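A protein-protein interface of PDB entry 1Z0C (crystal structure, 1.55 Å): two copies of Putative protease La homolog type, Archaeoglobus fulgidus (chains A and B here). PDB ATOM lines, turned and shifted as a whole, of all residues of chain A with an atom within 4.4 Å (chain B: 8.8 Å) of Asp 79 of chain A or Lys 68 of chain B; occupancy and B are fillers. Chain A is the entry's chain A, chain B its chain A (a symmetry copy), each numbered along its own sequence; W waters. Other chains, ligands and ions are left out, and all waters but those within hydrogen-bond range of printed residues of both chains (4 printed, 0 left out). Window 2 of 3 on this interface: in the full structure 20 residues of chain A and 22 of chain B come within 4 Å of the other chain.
The side-chain carboxylate (OE1) of Glu 34 of chain A is in salt-bridge range of the side-chain amino group (NZ) of Lys 69 of chain B (3.0 Å). The side-chain amino group (NZ) of Lys 69 of chain B lies within hydrogen-bond range of the backbone carbonyl oxygen (O) of Val 35 of chain A (2.7 Å). The side-chain carboxylate of Asp 79 of chain A is in salt-bridge range of the side-chain amino group of Lys 68 of chain B (2.8 Å). A ring nitrogen (ND1) of His 81 of chain A lies close to the backbone carbonyl oxygen (O) of Met 61 of chain B (3.4 Å). A ring nitrogen (NE2) of His 81 of chain A sits at hydrogen-bond distance from the side-chain amino group (NZ) of Lys 68 of chain B, 3.0 Å away.
O of Glu 34 of chain A is in hydrogen-bond range of N of His 81 of chain A. The backbone carbonyl oxygen (O) of Met 78 of chain A sits at hydrogen-bond distance from the backbone NH (N) of Arg 45 of chain A, at 3.5 Å. OD1 of Asp 79 of chain A lies within hydrogen-bond range of N of Arg 45 of chain A, 2.9 Å away. O of Arg 45 of chain A is in hydrogen-bond range of N of Val 80 of chain A (2.9 Å). The backbone carbonyl oxygen (O) of Val 80 of chain A is in hydrogen-bond range of the backbone NH (N) of Ile 47 of chain A, at 2.8 Å. ND2 of Asn 77 of chain B lies close to OD1 of Asp 74 of chain B.
Val 125 of chain B touches Glu 34 of chain A (O to CG, 3.7 Å). Thr 36 of chain A touches Ala 65 of chain B. OG1 of Thr 36 of chain A touches CE of Lys 68 of chain B, at 3.6 Å. Met 39 of chain A touches Gly 72 of chain B (CE to O, 2.8 Å). OD1 of Asp 74 of chain B touches CB of Met 39 of chain A, at 3.9 Å. Arg 45 of chain A touches Ser 76 of chain B. CG2 of Ile 47 of chain A touches CE of Met 61 of chain B, 3.4 Å away. Lys 68 of chain B touches Ile 47 of chain A. Ala 65 of chain B touches His 81 of chain A (CB to NE2, 3.6 Å).
Of chain B, only Lys 68 comes within 4 Å of Asp 79 of chain A. Of chain A, only Thr 36 (3.6 Å), Ile 47 (3.6 Å), Asp 79 (2.8 Å) and His 81 (3.0 Å) come within 4 Å of Lys 68 of chain B. Of chain B, only Ala 65 (3.6 Å) and Lys 68 (3.6 Å) come within 4 Å of Thr 36 of chain A. Of the printed residues of chain A, Asp 74 of chain B touches Met 39 (3.9 Å). Of the printed residues of chain A, Ala 65 of chain B touches Thr 36 (3.6 Å) and His 81 (3.6 Å). Glu 109 of chain B touches none of the printed residues of chain A. The nearest residue of chain A that does not touch Lys 68 of chain B is Met 39 of chain A (4.1 Å). The nearest printed residue of chain A that does not touch Ser 76 of chain B is Asp 79 of chain A (4.2 Å).
Printed residues of chain A that touch a printed residue of chain B: Glu 34, Val 35, Thr 36, Met 39, Arg 45, Ile 47, Asp 79 and His 81. Hydrophobic or aromatic side chains of chain A that line the printed part of chain B: Met 39, Ile 47 and His 81. Of the 24 printed residues of chain B, 8 touch a printed residue of chain A. Hydrophobic or aromatic side chains of chain B that line the printed part of chain A: Met 61, Ala 65 and Val 125.
No position is printed for both chains. Of the 14 pairs that touch across the chains among the printed residues, none has its exchanged pair printed and touching as well.
Water W3 bridges OH of Tyr 70 of chain B (2.7 Å) and OE2 of Glu 34 of chain A (3.4 Å). Water W2 lies within hydrogen-bond range of the side-chain carboxylate (OD2) of Asp 79 of chain A (2.7 Å), the side-chain hydroxyl (OG) of Ser 76 of chain B (3.0 Å) and the backbone carbonyl oxygen (O) of Ser 38 of chain A (3.3 Å). Water W1 lies within hydrogen-bond range of O of Val 125 of chain B (2.7 Å) and OE2 of Glu 34 of chain A (3.0 Å). Water W4 lies within hydrogen-bond range of a ring nitrogen (ND1) of His 81 of chain A (2.9 Å), the side-chain amide oxygen of Asn 62 of chain B (3.0 Å) and the backbone carbonyl oxygen of Met 61 of chain B (3.5 Å).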
ATOM      1  N   GLU A  34     -19.033  -2.287  19.180  1.00  0.00           N
ATOM      2  CA  GLU A  34     -20.266  -2.899  19.670  1.00  0.00           C
ATOM      3  C   GLU A  34     -21.001  -3.384  18.433  1.00  0.00           C
ATOM      4  O   GLU A  34     -20.932  -2.762  17.388  1.00  0.00           O
ATOM      5  CB  GLU A  34     -21.141  -1.909  20.450  1.00  0.00           C
ATOM      6  CG  GLU A  34     -22.378  -2.539  21.092  1.00  0.00           C
ATOM      7  CD  GLU A  34     -22.068  -3.814  21.915  1.00  0.00           C
ATOM      8  OE1 GLU A  34     -21.731  -4.898  21.398  1.00  0.00           O
ATOM      9  OE2 GLU A  34     -22.125  -3.705  23.133  1.00  0.00           O
ATOM     10  N   VAL A  35     -21.662  -4.522  18.574  1.00  0.00           N
ATOM     11  CA  VAL A  35     -22.474  -5.061  17.507  1.00  0.00           C
ATOM     12  C   VAL A  35     -23.900  -5.226  18.043  1.00  0.00           C
ATOM     13  O   VAL A  35     -24.086  -5.548  19.216  1.00  0.00           O
ATOM     14  CB  VAL A  35     -21.886  -6.376  17.018  1.00  0.00           C
ATOM     15  CG1 VAL A  35     -20.446  -6.159  16.525  1.00  0.00           C
ATOM     16  CG2 VAL A  35     -22.009  -7.460  18.089  1.00  0.00           C
ATOM     17  N   THR A  36     -24.870  -4.801  17.237  1.00  0.00           N
ATOM     18  CA  THR A  36     -26.287  -4.941  17.602  1.00  0.00           C
ATOM     19  C   THR A  36     -27.044  -5.601  16.444  1.00  0.00           C
ATOM     20  O   THR A  36     -26.691  -5.432  15.297  1.00  0.00           O
ATOM     21  CB  THR A  36     -26.951  -3.544  17.842  1.00  0.00           C
ATOM     22  OG1 THR A  36     -27.134  -2.854  16.603  1.00  0.00           O
ATOM     23  CG2 THR A  36     -26.043  -2.655  18.684  1.00  0.00           C
ATOM     24  N   PRO A  37     -28.158  -6.313  16.740  1.00  0.00           N
ATOM     25  CA  PRO A  37     -29.004  -6.692  15.607  1.00  0.00           C
ATOM     26  C   PRO A  37     -29.382  -5.449  14.797  1.00  0.00           C
ATOM     27  O   PRO A  37     -29.472  -4.338  15.330  1.00  0.00           O
ATOM     28  CB  PRO A  37     -30.267  -7.249  16.270  1.00  0.00           C
ATOM     29  CG  PRO A  37     -29.931  -7.529  17.673  1.00  0.00           C
ATOM     30  CD  PRO A  37     -28.681  -6.754  18.034  1.00  0.00           C
ATOM     31  N   SER A  38     -29.579  -5.629  13.502  1.00  0.00           N
ATOM     32  CA  SER A  38     -29.942  -4.520  12.644  1.00  0.00           C
ATOM     33  C   SER A  38     -31.430  -4.151  12.700  1.00  0.00           C
ATOM     34  O   SER A  38     -31.878  -3.293  11.940  1.00  0.00           O
ATOM     35  CB  SER A  38     -29.519  -4.823  11.209  1.00  0.00           C
ATOM     36  OG  SER A  38     -29.963  -6.117  10.812  1.00  0.00           O
ATOM     37  N   MET A  39     -32.175  -4.794  13.602  1.00  0.00           N
ATOM     38  CA  MET A  39     -33.590  -4.455  13.914  1.00  0.00           C
ATOM     39  C   MET A  39     -34.529  -4.769  12.746  1.00  0.00           C
ATOM     40  O   MET A  39     -35.013  -3.859  12.063  1.00  0.00           O
ATOM     41  CB  MET A  39     -33.769  -2.982  14.351  1.00  0.00           C
ATOM     42  CG  MET A  39     -32.720  -2.431  15.359  1.00  0.00           C
ATOM     43  SD  MET A  39     -32.998  -2.909  17.089  1.00  0.00           S
ATOM     44  CE  MET A  39     -34.741  -2.546  17.224  1.00  0.00           C
ATOM     45  N   GLY A  44     -27.671  -4.737   7.935  1.00  0.00           N
ATOM     46  CA  GLY A  44     -26.845  -4.050   8.902  1.00  0.00           C
ATOM     47  C   GLY A  44     -25.970  -2.979   8.308  1.00  0.00           C
ATOM     48  O   GLY A  44     -25.670  -2.971   7.109  1.00  0.00           O
ATOM     49  N   ARG A  45     -25.547  -2.079   9.183  1.00  0.00           N
ATOM     50  CA  ARG A  45     -24.760  -0.912   8.848  1.00  0.00           C
ATOM     51  C   ARG A  45     -23.447  -0.932   9.640  1.00  0.00           C
ATOM     52  O   ARG A  45     -23.404  -1.518  10.709  1.00  0.00           O
ATOM     53  CB  ARG A  45     -25.580   0.312   9.211  1.00  0.00           C
ATOM     54  CG  ARG A  45     -26.632   0.617   8.124  1.00  0.00           C
ATOM     55  CD  ARG A  45     -27.924   1.264   8.615  1.00  0.00           C
ATOM     56  NE  ARG A  45     -28.744   1.648   7.454  1.00  0.00           N
ATOM     57  CZ  ARG A  45     -29.905   2.303   7.503  1.00  0.00           C
ATOM     58  NH1 ARG A  45     -30.441   2.684   8.665  1.00  0.00           N
ATOM     59  NH2 ARG A  45     -30.535   2.586   6.366  1.00  0.00           N
ATOM     60  N   ILE A  47     -21.302   1.706  11.517  1.00  0.00           N
ATOM     61  CA  ILE A  47     -21.481   3.051  12.004  1.00  0.00           C
ATOM     62  C   ILE A  47     -20.193   3.564  12.637  1.00  0.00           C
ATOM     63  O   ILE A  47     -19.694   2.985  13.573  1.00  0.00           O
ATOM     64  CB  ILE A  47     -22.644   3.104  12.953  1.00  0.00           C
ATOM     65  CG1 ILE A  47     -23.920   2.717  12.181  1.00  0.00           C
ATOM     66  CG2 ILE A  47     -22.758   4.494  13.495  1.00  0.00           C
ATOM     67  CD1 ILE A  47     -25.021   2.175  13.020  1.00  0.00           C
ATOM     68  N   MET A  78     -26.169  -7.252  11.124  1.00  0.00           N
ATOM     69  CA  MET A  78     -25.800  -6.696  12.419  1.00  0.00           C
ATOM     70  C   MET A  78     -25.410  -5.289  12.136  1.00  0.00           C
ATOM     71  O   MET A  78     -24.926  -4.991  11.019  1.00  0.00           O
ATOM     72  CB  MET A  78     -24.587  -7.424  13.000  1.00  0.00           C
ATOM     73  CG  MET A  78     -24.797  -8.910  13.295  1.00  0.00           C
ATOM     74  SD  MET A  78     -23.296  -9.487  14.106  1.00  0.00           S
ATOM     75  CE  MET A  78     -23.640 -11.236  14.310  1.00  0.00           C
ATOM     76  N   ASP A  79     -25.628  -4.395  13.113  1.00  0.00           N
ATOM     77  CA  ASP A  79     -25.047  -3.050  13.022  1.00  0.00           C
ATOM     78  C   ASP A  79     -23.721  -3.161  13.807  1.00  0.00           C
ATOM     79  O   ASP A  79     -23.713  -3.697  14.892  1.00  0.00           O
ATOM     80  CB  ASP A  79     -25.922  -1.998  13.678  1.00  0.00           C
ATOM     81  CG  ASP A  79     -27.122  -1.619  12.796  1.00  0.00           C
ATOM     82  OD1 ASP A  79     -27.158  -2.012  11.598  1.00  0.00           O
ATOM     83  OD2 ASP A  79     -27.975  -0.889  13.297  1.00  0.00           O
ATOM     84  N   VAL A  80     -22.655  -2.645  13.222  1.00  0.00           N
ATOM     85  CA  VAL A  80     -21.322  -2.647  13.857  1.00  0.00           C
ATOM     86  C   VAL A  80     -20.915  -1.225  14.114  1.00  0.00           C
ATOM     87  O   VAL A  80     -20.747  -0.446  13.185  1.00  0.00           O
ATOM     88  CB  VAL A  80     -20.264  -3.298  12.925  1.00  0.00           C
ATOM     89  CG1 VAL A  80     -18.835  -3.354  13.564  1.00  0.00           C
ATOM     90  CG2 VAL A  80     -20.713  -4.736  12.568  1.00  0.00           C
ATOM     91  N   HIS A  81     -20.755  -0.896  15.387  1.00  0.00           N
ATOM     92  CA  HIS A  81     -20.346   0.443  15.783  1.00  0.00           C
ATOM     93  C   HIS A  81     -18.875   0.494  16.135  1.00  0.00           C
ATOM     94  O   HIS A  81     -18.469  -0.307  16.977  1.00  0.00           O
ATOM     95  CB  HIS A  81     -21.115   0.922  17.030  1.00  0.00           C
ATOM     96  CG  HIS A  81     -22.571   1.147  16.801  1.00  0.00           C
ATOM     97  ND1 HIS A  81     -23.144   2.402  16.771  1.00  0.00           N
ATOM     98  CD2 HIS A  81     -23.562   0.264  16.581  1.00  0.00           C
ATOM     99  CE1 HIS A  81     -24.447   2.275  16.545  1.00  0.00           C
ATOM    100  NE2 HIS A  81     -24.730   0.988  16.444  1.00  0.00           N
ATOM    101  N   VAL B  60     -24.596  10.805  19.308  1.00  0.00           N
ATOM    102  CA  VAL B  60     -25.854  10.144  18.991  1.00  0.00           C
ATOM    103  C   VAL B  60     -25.588   8.725  18.438  1.00  0.00           C
ATOM    104  O   VAL B  60     -26.334   7.836  18.774  1.00  0.00           O
ATOM    105  CB  VAL B  60     -26.695  10.946  18.013  1.00  0.00           C
ATOM    106  CG1 VAL B  60     -27.940  10.237  17.626  1.00  0.00           C
ATOM    107  CG2 VAL B  60     -27.096  12.318  18.706  1.00  0.00           C
ATOM    108  N   MET B  61     -24.551   8.557  17.641  1.00  0.00           N
ATOM    109  CA  MET B  61     -24.302   7.199  17.134  1.00  0.00           C
ATOM    110  C   MET B  61     -23.923   6.275  18.248  1.00  0.00           C
ATOM    111  O   MET B  61     -24.380   5.122  18.291  1.00  0.00           O
ATOM    112  CB  MET B  61     -23.254   7.229  16.041  1.00  0.00           C
ATOM    113  CG  MET B  61     -23.746   8.026  14.833  1.00  0.00           C
ATOM    114  SD  MET B  61     -25.504   7.905  14.227  1.00  0.00           S
ATOM    115  CE  MET B  61     -25.687   6.155  13.977  1.00  0.00           C
ATOM    116  N   ASN B  62     -23.129   6.756  19.207  1.00  0.00           N
ATOM    117  CA  ASN B  62     -22.766   5.833  20.306  1.00  0.00           C
ATOM    118  C   ASN B  62     -23.941   5.472  21.178  1.00  0.00           C
ATOM    119  O   ASN B  62     -24.122   4.322  21.622  1.00  0.00           O
ATOM    120  CB  ASN B  62     -21.667   6.443  21.190  1.00  0.00           C
ATOM    121  CG  ASN B  62     -20.345   6.526  20.504  1.00  0.00           C
ATOM    122  OD1 ASN B  62     -20.189   6.228  19.304  1.00  0.00           O
ATOM    123  ND2 ASN B  62     -19.375   7.003  21.260  1.00  0.00           N
ATOM    124  N   VAL B  63     -24.780   6.468  21.501  1.00  0.00           N
ATOM    125  CA  VAL B  63     -25.916   6.111  22.336  1.00  0.00           C
ATOM    126  C   VAL B  63     -26.888   5.267  21.527  1.00  0.00           C
ATOM    127  O   VAL B  63     -27.593   4.441  22.128  1.00  0.00           O
ATOM    128  CB  VAL B  63     -26.572   7.319  22.991  1.00  0.00           C
ATOM    129  CG1 VAL B  63     -27.421   8.126  21.959  1.00  0.00           C
ATOM    130  CG2 VAL B  63     -27.398   6.897  24.229  1.00  0.00           C
ATOM    131  N   SER B  64     -26.865   5.362  20.195  1.00  0.00           N
ATOM    132  CA  SER B  64     -27.781   4.539  19.411  1.00  0.00           C
ATOM    133  C   SER B  64     -27.440   3.059  19.597  1.00  0.00           C
ATOM    134  O   SER B  64     -28.317   2.214  19.669  1.00  0.00           O
ATOM    135  CB  SER B  64     -27.713   4.963  17.947  1.00  0.00           C
ATOM    136  OG  SER B  64     -28.309   6.263  17.749  1.00  0.00           O
ATOM    137  N   ALA B  65     -26.145   2.756  19.716  1.00  0.00           N
ATOM    138  CA  ALA B  65     -25.821   1.367  19.924  1.00  0.00           C
ATOM    139  C   ALA B  65     -26.494   0.811  21.178  1.00  0.00           C
ATOM    140  O   ALA B  65     -26.996  -0.314  21.188  1.00  0.00           O
ATOM    141  CB  ALA B  65     -24.310   1.239  20.034  1.00  0.00           C
ATOM    142  N   ILE B  66     -26.416   1.594  22.248  1.00  0.00           N
ATOM    143  CA  ILE B  66     -26.944   1.187  23.541  1.00  0.00           C
ATOM    144  C   ILE B  66     -28.477   1.158  23.510  1.00  0.00           C
ATOM    145  O   ILE B  66     -29.097   0.229  24.087  1.00  0.00           O
ATOM    146  CB  ILE B  66     -26.459   2.177  24.644  1.00  0.00           C
ATOM    147  CG1 ILE B  66     -24.926   2.081  24.844  1.00  0.00           C
ATOM    148  CG2 ILE B  66     -27.111   1.815  25.969  1.00  0.00           C
ATOM    149  CD1 ILE B  66     -24.299   3.403  25.308  1.00  0.00           C
ATOM    150  N   ILE B  67     -29.076   2.111  22.809  1.00  0.00           N
ATOM    151  CA  ILE B  67     -30.538   2.176  22.705  1.00  0.00           C
ATOM    152  C   ILE B  67     -31.012   0.923  21.932  1.00  0.00           C
ATOM    153  O   ILE B  67     -32.006   0.271  22.383  1.00  0.00           O
ATOM    154  CB  ILE B  67     -30.965   3.479  22.075  1.00  0.00           C
ATOM    155  CG1 ILE B  67     -30.693   4.639  23.031  1.00  0.00           C
ATOM    156  CG2 ILE B  67     -32.482   3.417  21.628  1.00  0.00           C
ATOM    157  CD1 ILE B  67     -30.812   5.996  22.343  1.00  0.00           C
ATOM    158  N   LYS B  68     -30.322   0.549  20.848  1.00  0.00           N
ATOM    159  CA  LYS B  68     -30.728  -0.648  20.089  1.00  0.00           C
ATOM    160  C   LYS B  68     -30.513  -1.935  20.872  1.00  0.00           C
ATOM    161  O   LYS B  68     -31.400  -2.802  20.934  1.00  0.00           O
ATOM    162  CB  LYS B  68     -29.982  -0.739  18.745  1.00  0.00           C
ATOM    163  CG  LYS B  68     -30.383   0.304  17.732  1.00  0.00           C
ATOM    164  CD  LYS B  68     -29.621   0.224  16.420  1.00  0.00           C
ATOM    165  CE  LYS B  68     -28.168   0.572  16.661  1.00  0.00           C
ATOM    166  NZ  LYS B  68     -27.480   0.853  15.371  1.00  0.00           N
ATOM    167  N   LYS B  69     -29.343  -2.068  21.498  1.00  0.00           N
ATOM    168  CA  LYS B  69     -28.980  -3.288  22.191  1.00  0.00           C
ATOM    169  C   LYS B  69     -29.902  -3.558  23.373  1.00  0.00           C
ATOM    170  O   LYS B  69     -30.351  -4.699  23.569  1.00  0.00           O
ATOM    171  CB  LYS B  69     -27.524  -3.215  22.687  1.00  0.00           C
ATOM    172  CG  LYS B  69     -26.883  -4.611  23.016  1.00  0.00           C
ATOM    173  CD  LYS B  69     -25.347  -4.602  22.913  1.00  0.00           C
ATOM    174  CE  LYS B  69     -24.619  -6.055  22.931  1.00  0.00           C
ATOM    175  NZ  LYS B  69     -24.036  -6.804  21.645  1.00  0.00           N
ATOM    176  N   TYR B  70     -30.215  -2.540  24.151  1.00  0.00           N
ATOM    177  CA  TYR B  70     -30.841  -2.788  25.472  1.00  0.00           C
ATOM    178  C   TYR B  70     -32.341  -2.470  25.549  1.00  0.00           C
ATOM    179  O   TYR B  70     -33.084  -3.070  26.344  1.00  0.00           O
ATOM    180  CB  TYR B  70     -30.056  -2.037  26.580  1.00  0.00           C
ATOM    181  CG  TYR B  70     -28.684  -2.622  26.758  1.00  0.00           C
ATOM    182  CD1 TYR B  70     -28.518  -3.847  27.412  1.00  0.00           C
ATOM    183  CD2 TYR B  70     -27.552  -1.963  26.288  1.00  0.00           C
ATOM    184  CE1 TYR B  70     -27.245  -4.418  27.584  1.00  0.00           C
ATOM    185  CE2 TYR B  70     -26.282  -2.526  26.432  1.00  0.00           C
ATOM    186  CZ  TYR B  70     -26.144  -3.736  27.099  1.00  0.00           C
ATOM    187  OH  TYR B  70     -24.889  -4.303  27.248  1.00  0.00           O
ATOM    188  N   THR B  71     -32.794  -1.536  24.722  1.00  0.00           N
ATOM    189  CA  THR B  71     -34.201  -1.112  24.813  1.00  0.00           C
ATOM    190  C   THR B  71     -34.979  -1.513  23.541  1.00  0.00           C
ATOM    191  O   THR B  71     -36.221  -1.476  23.490  1.00  0.00           O
ATOM    192  CB  THR B  71     -34.333   0.424  25.102  1.00  0.00           C
ATOM    193  OG1 THR B  71     -34.014   1.182  23.933  1.00  0.00           O
ATOM    194  CG2 THR B  71     -33.449   0.879  26.258  1.00  0.00           C
ATOM    195  N   GLY B  72     -34.246  -1.858  22.498  1.00  0.00           N
ATOM    196  CA  GLY B  72     -34.847  -2.259  21.244  1.00  0.00           C
ATOM    197  C   GLY B  72     -35.533  -1.176  20.431  1.00  0.00           C
ATOM    198  O   GLY B  72     -36.194  -1.514  19.427  1.00  0.00           O
ATOM    199  N   ARG B  73     -35.404   0.098  20.833  1.00  0.00           N
ATOM    200  CA  ARG B  73     -35.943   1.239  20.028  1.00  0.00           C
ATOM    201  C   ARG B  73     -35.281   1.385  18.660  1.00  0.00           C
ATOM    202  O   ARG B  73     -34.046   1.298  18.532  1.00  0.00           O
ATOM    203  CB  ARG B  73     -35.886   2.580  20.784  1.00  0.00           C
ATOM    204  CG  ARG B  73     -36.561   2.579  22.155  1.00  0.00           C
ATOM    205  CD  ARG B  73     -37.889   3.292  22.148  1.00  0.00           C
ATOM    206  NE  ARG B  73     -38.423   3.348  23.495  1.00  0.00           N
ATOM    207  CZ  ARG B  73     -39.657   3.733  23.809  1.00  0.00           C
ATOM    208  NH1 ARG B  73     -40.518   4.098  22.866  1.00  0.00           N
ATOM    209  NH2 ARG B  73     -40.038   3.746  25.079  1.00  0.00           N
ATOM    210  N   ASP B  74     -36.112   1.616  17.635  1.00  0.00           N
ATOM    211  CA  ASP B  74     -35.639   1.700  16.253  1.00  0.00           C
ATOM    212  C   ASP B  74     -35.105   3.079  15.878  1.00  0.00           C
ATOM    213  O   ASP B  74     -35.721   3.824  15.094  1.00  0.00           O
ATOM    214  CB  ASP B  74     -36.709   1.270  15.232  1.00  0.00           C
ATOM    215  CG  ASP B  74     -36.110   1.065  13.859  1.00  0.00           C
ATOM    216  OD1 ASP B  74     -34.889   0.753  13.779  1.00  0.00           O
ATOM    217  OD2 ASP B  74     -36.830   1.246  12.861  1.00  0.00           O
ATOM    218  N   ILE B  75     -33.946   3.409  16.420  1.00  0.00           N
ATOM    219  CA  ILE B  75     -33.431   4.776  16.309  1.00  0.00           C
ATOM    220  C   ILE B  75     -32.885   5.097  14.908  1.00  0.00           C
ATOM    221  O   ILE B  75     -32.845   6.254  14.500  1.00  0.00           O
ATOM    222  CB  ILE B  75     -32.431   5.058  17.444  1.00  0.00           C
ATOM    223  CG1 ILE B  75     -32.125   6.553  17.539  1.00  0.00           C
ATOM    224  CG2 ILE B  75     -31.184   4.261  17.226  1.00  0.00           C
ATOM    225  CD1 ILE B  75     -31.525   6.920  18.890  1.00  0.00           C
ATOM    226  N   SER B  76     -32.540   4.063  14.134  1.00  0.00           N
ATOM    227  CA  SER B  76     -32.122   4.275  12.759  1.00  0.00           C
ATOM    228  C   SER B  76     -33.266   4.801  11.909  1.00  0.00           C
ATOM    229  O   SER B  76     -33.033   5.388  10.856  1.00  0.00           O
ATOM    230  CB  SER B  76     -31.550   2.992  12.141  1.00  0.00           C
ATOM    231  OG  SER B  76     -30.453   2.536  12.915  1.00  0.00           O
ATOM    232  N   ASN B  77     -34.495   4.598  12.378  1.00  0.00           N
ATOM    233  CA  ASN B  77     -35.702   5.112  11.708  1.00  0.00           C
ATOM    234  C   ASN B  77     -36.348   6.308  12.461  1.00  0.00           C
ATOM    235  O   ASN B  77     -37.563   6.433  12.618  1.00  0.00           O
ATOM    236  CB  ASN B  77     -36.695   3.976  11.460  1.00  0.00           C
ATOM    237  CG  ASN B  77     -36.188   2.990  10.422  1.00  0.00           C
ATOM    238  OD1 ASN B  77     -36.023   3.331   9.244  1.00  0.00           O
ATOM    239  ND2 ASN B  77     -35.899   1.769  10.858  1.00  0.00           N
ATOM    240  N   ILE B 105     -31.876   9.854  25.127  1.00  0.00           N
ATOM    241  CA  ILE B 105     -32.620   8.824  25.843  1.00  0.00           C
ATOM    242  C   ILE B 105     -33.861   9.488  26.467  1.00  0.00           C
ATOM    243  O   ILE B 105     -34.963   8.918  26.344  1.00  0.00           O
ATOM    244  CB  ILE B 105     -31.737   8.192  26.946  1.00  0.00           C
ATOM    245  CG1 ILE B 105     -30.681   7.370  26.239  1.00  0.00           C
ATOM    246  CG2 ILE B 105     -32.616   7.308  27.865  1.00  0.00           C
ATOM    247  CD1 ILE B 105     -29.555   6.910  27.174  1.00  0.00           C
ATOM    248  N   ILE B 108     -36.424  10.239  23.684  1.00  0.00           N
ATOM    249  CA  ILE B 108     -37.081   9.056  23.083  1.00  0.00           C
ATOM    250  C   ILE B 108     -38.064   8.454  24.036  1.00  0.00           C
ATOM    251  O   ILE B 108     -39.152   8.021  23.588  1.00  0.00           O
ATOM    252  CB  ILE B 108     -36.060   7.967  22.679  1.00  0.00           C
ATOM    253  CG1 ILE B 108     -35.253   8.422  21.510  1.00  0.00           C
ATOM    254  CG2 ILE B 108     -36.837   6.711  22.270  1.00  0.00           C
ATOM    255  CD1 ILE B 108     -34.055   7.533  21.272  1.00  0.00           C
ATOM    256  N   GLU B 109     -37.694   8.427  25.323  1.00  0.00           N
ATOM    257  CA  GLU B 109     -38.484   7.760  26.342  1.00  0.00           C
ATOM    258  C   GLU B 109     -39.532   8.683  26.945  1.00  0.00           C
ATOM    259  O   GLU B 109     -40.422   8.162  27.689  1.00  0.00           O
ATOM    260  CB  GLU B 109     -37.591   7.177  27.433  1.00  0.00           C
ATOM    261  CG  GLU B 109     -36.632   6.070  26.902  1.00  0.00           C
ATOM    262  CD  GLU B 109     -37.327   4.780  26.397  1.00  0.00           C
ATOM    263  OE1 GLU B 109     -38.439   4.450  26.902  1.00  0.00           O
ATOM    264  OE2 GLU B 109     -36.759   4.078  25.510  1.00  0.00           O
ATOM    265  N   VAL B 125     -19.451   3.121  23.299  1.00  0.00           N
ATOM    266  CA  VAL B 125     -20.500   2.369  22.581  1.00  0.00           C
ATOM    267  C   VAL B 125     -20.955   1.173  23.380  1.00  0.00           C
ATOM    268  O   VAL B 125     -22.039   0.575  23.086  1.00  0.00           O
ATOM    269  CB  VAL B 125     -20.094   1.932  21.157  1.00  0.00           C
ATOM    270  CG1 VAL B 125     -19.951   3.104  20.262  1.00  0.00           C
ATOM    271  CG2 VAL B 125     -18.755   1.134  21.160  1.00  0.00           C
ATOM    272  N   LYS B 198     -34.363  -2.414  31.833  1.00  0.00           N
ATOM    273  CA  LYS B 198     -33.781  -2.822  30.554  1.00  0.00           C
ATOM    274  C   LYS B 198     -32.264  -2.718  30.565  1.00  0.00           C
ATOM    275  O   LYS B 198     -31.595  -3.360  29.762  1.00  0.00           O
ATOM    276  CB  LYS B 198     -34.385  -2.024  29.389  1.00  0.00           C
ATOM    277  CG  LYS B 198     -35.847  -2.355  29.128  1.00  0.00           C
ATOM    278  CD  LYS B 198     -36.431  -1.544  27.996  1.00  0.00           C
ATOM    279  CE  LYS B 198     -37.810  -2.038  27.684  1.00  0.00           C
ATOM    280  NZ  LYS B 198     -38.603  -1.954  28.932  1.00  0.00           N
ATOM    281  N   PHE B 199     -31.727  -1.924  31.486  1.00  0.00           N
ATOM    282  CA  PHE B 199     -30.270  -1.756  31.619  1.00  0.00           C
ATOM    283  C   PHE B 199     -29.601  -2.714  32.605  1.00  0.00           C
ATOM    284  O   PHE B 199     -28.382  -2.725  32.731  1.00  0.00           O
ATOM    285  CB  PHE B 199     -29.940  -0.321  31.993  1.00  0.00           C
ATOM    286  CG  PHE B 199     -30.008   0.613  30.838  1.00  0.00           C
ATOM    287  CD1 PHE B 199     -29.027   0.600  29.852  1.00  0.00           C
ATOM    288  CD2 PHE B 199     -31.073   1.470  30.696  1.00  0.00           C
ATOM    289  CE1 PHE B 199     -29.108   1.451  28.763  1.00  0.00           C
ATOM    290  CE2 PHE B 199     -31.153   2.334  29.619  1.00  0.00           C
ATOM    291  CZ  PHE B 199     -30.172   2.319  28.641  1.00  0.00           C
HETATM  292  O   HOH W   1     -23.721  -1.334  24.101  1.00  0.00           O
HETATM  293  O   HOH W   2     -30.641  -0.422  13.056  1.00  0.00           O
HETATM  294  O   HOH W   3     -22.671  -3.096  26.444  1.00  0.00           O
HETATM  295  O   HOH W   4     -21.209   4.516  17.072  1.00  0.00           O
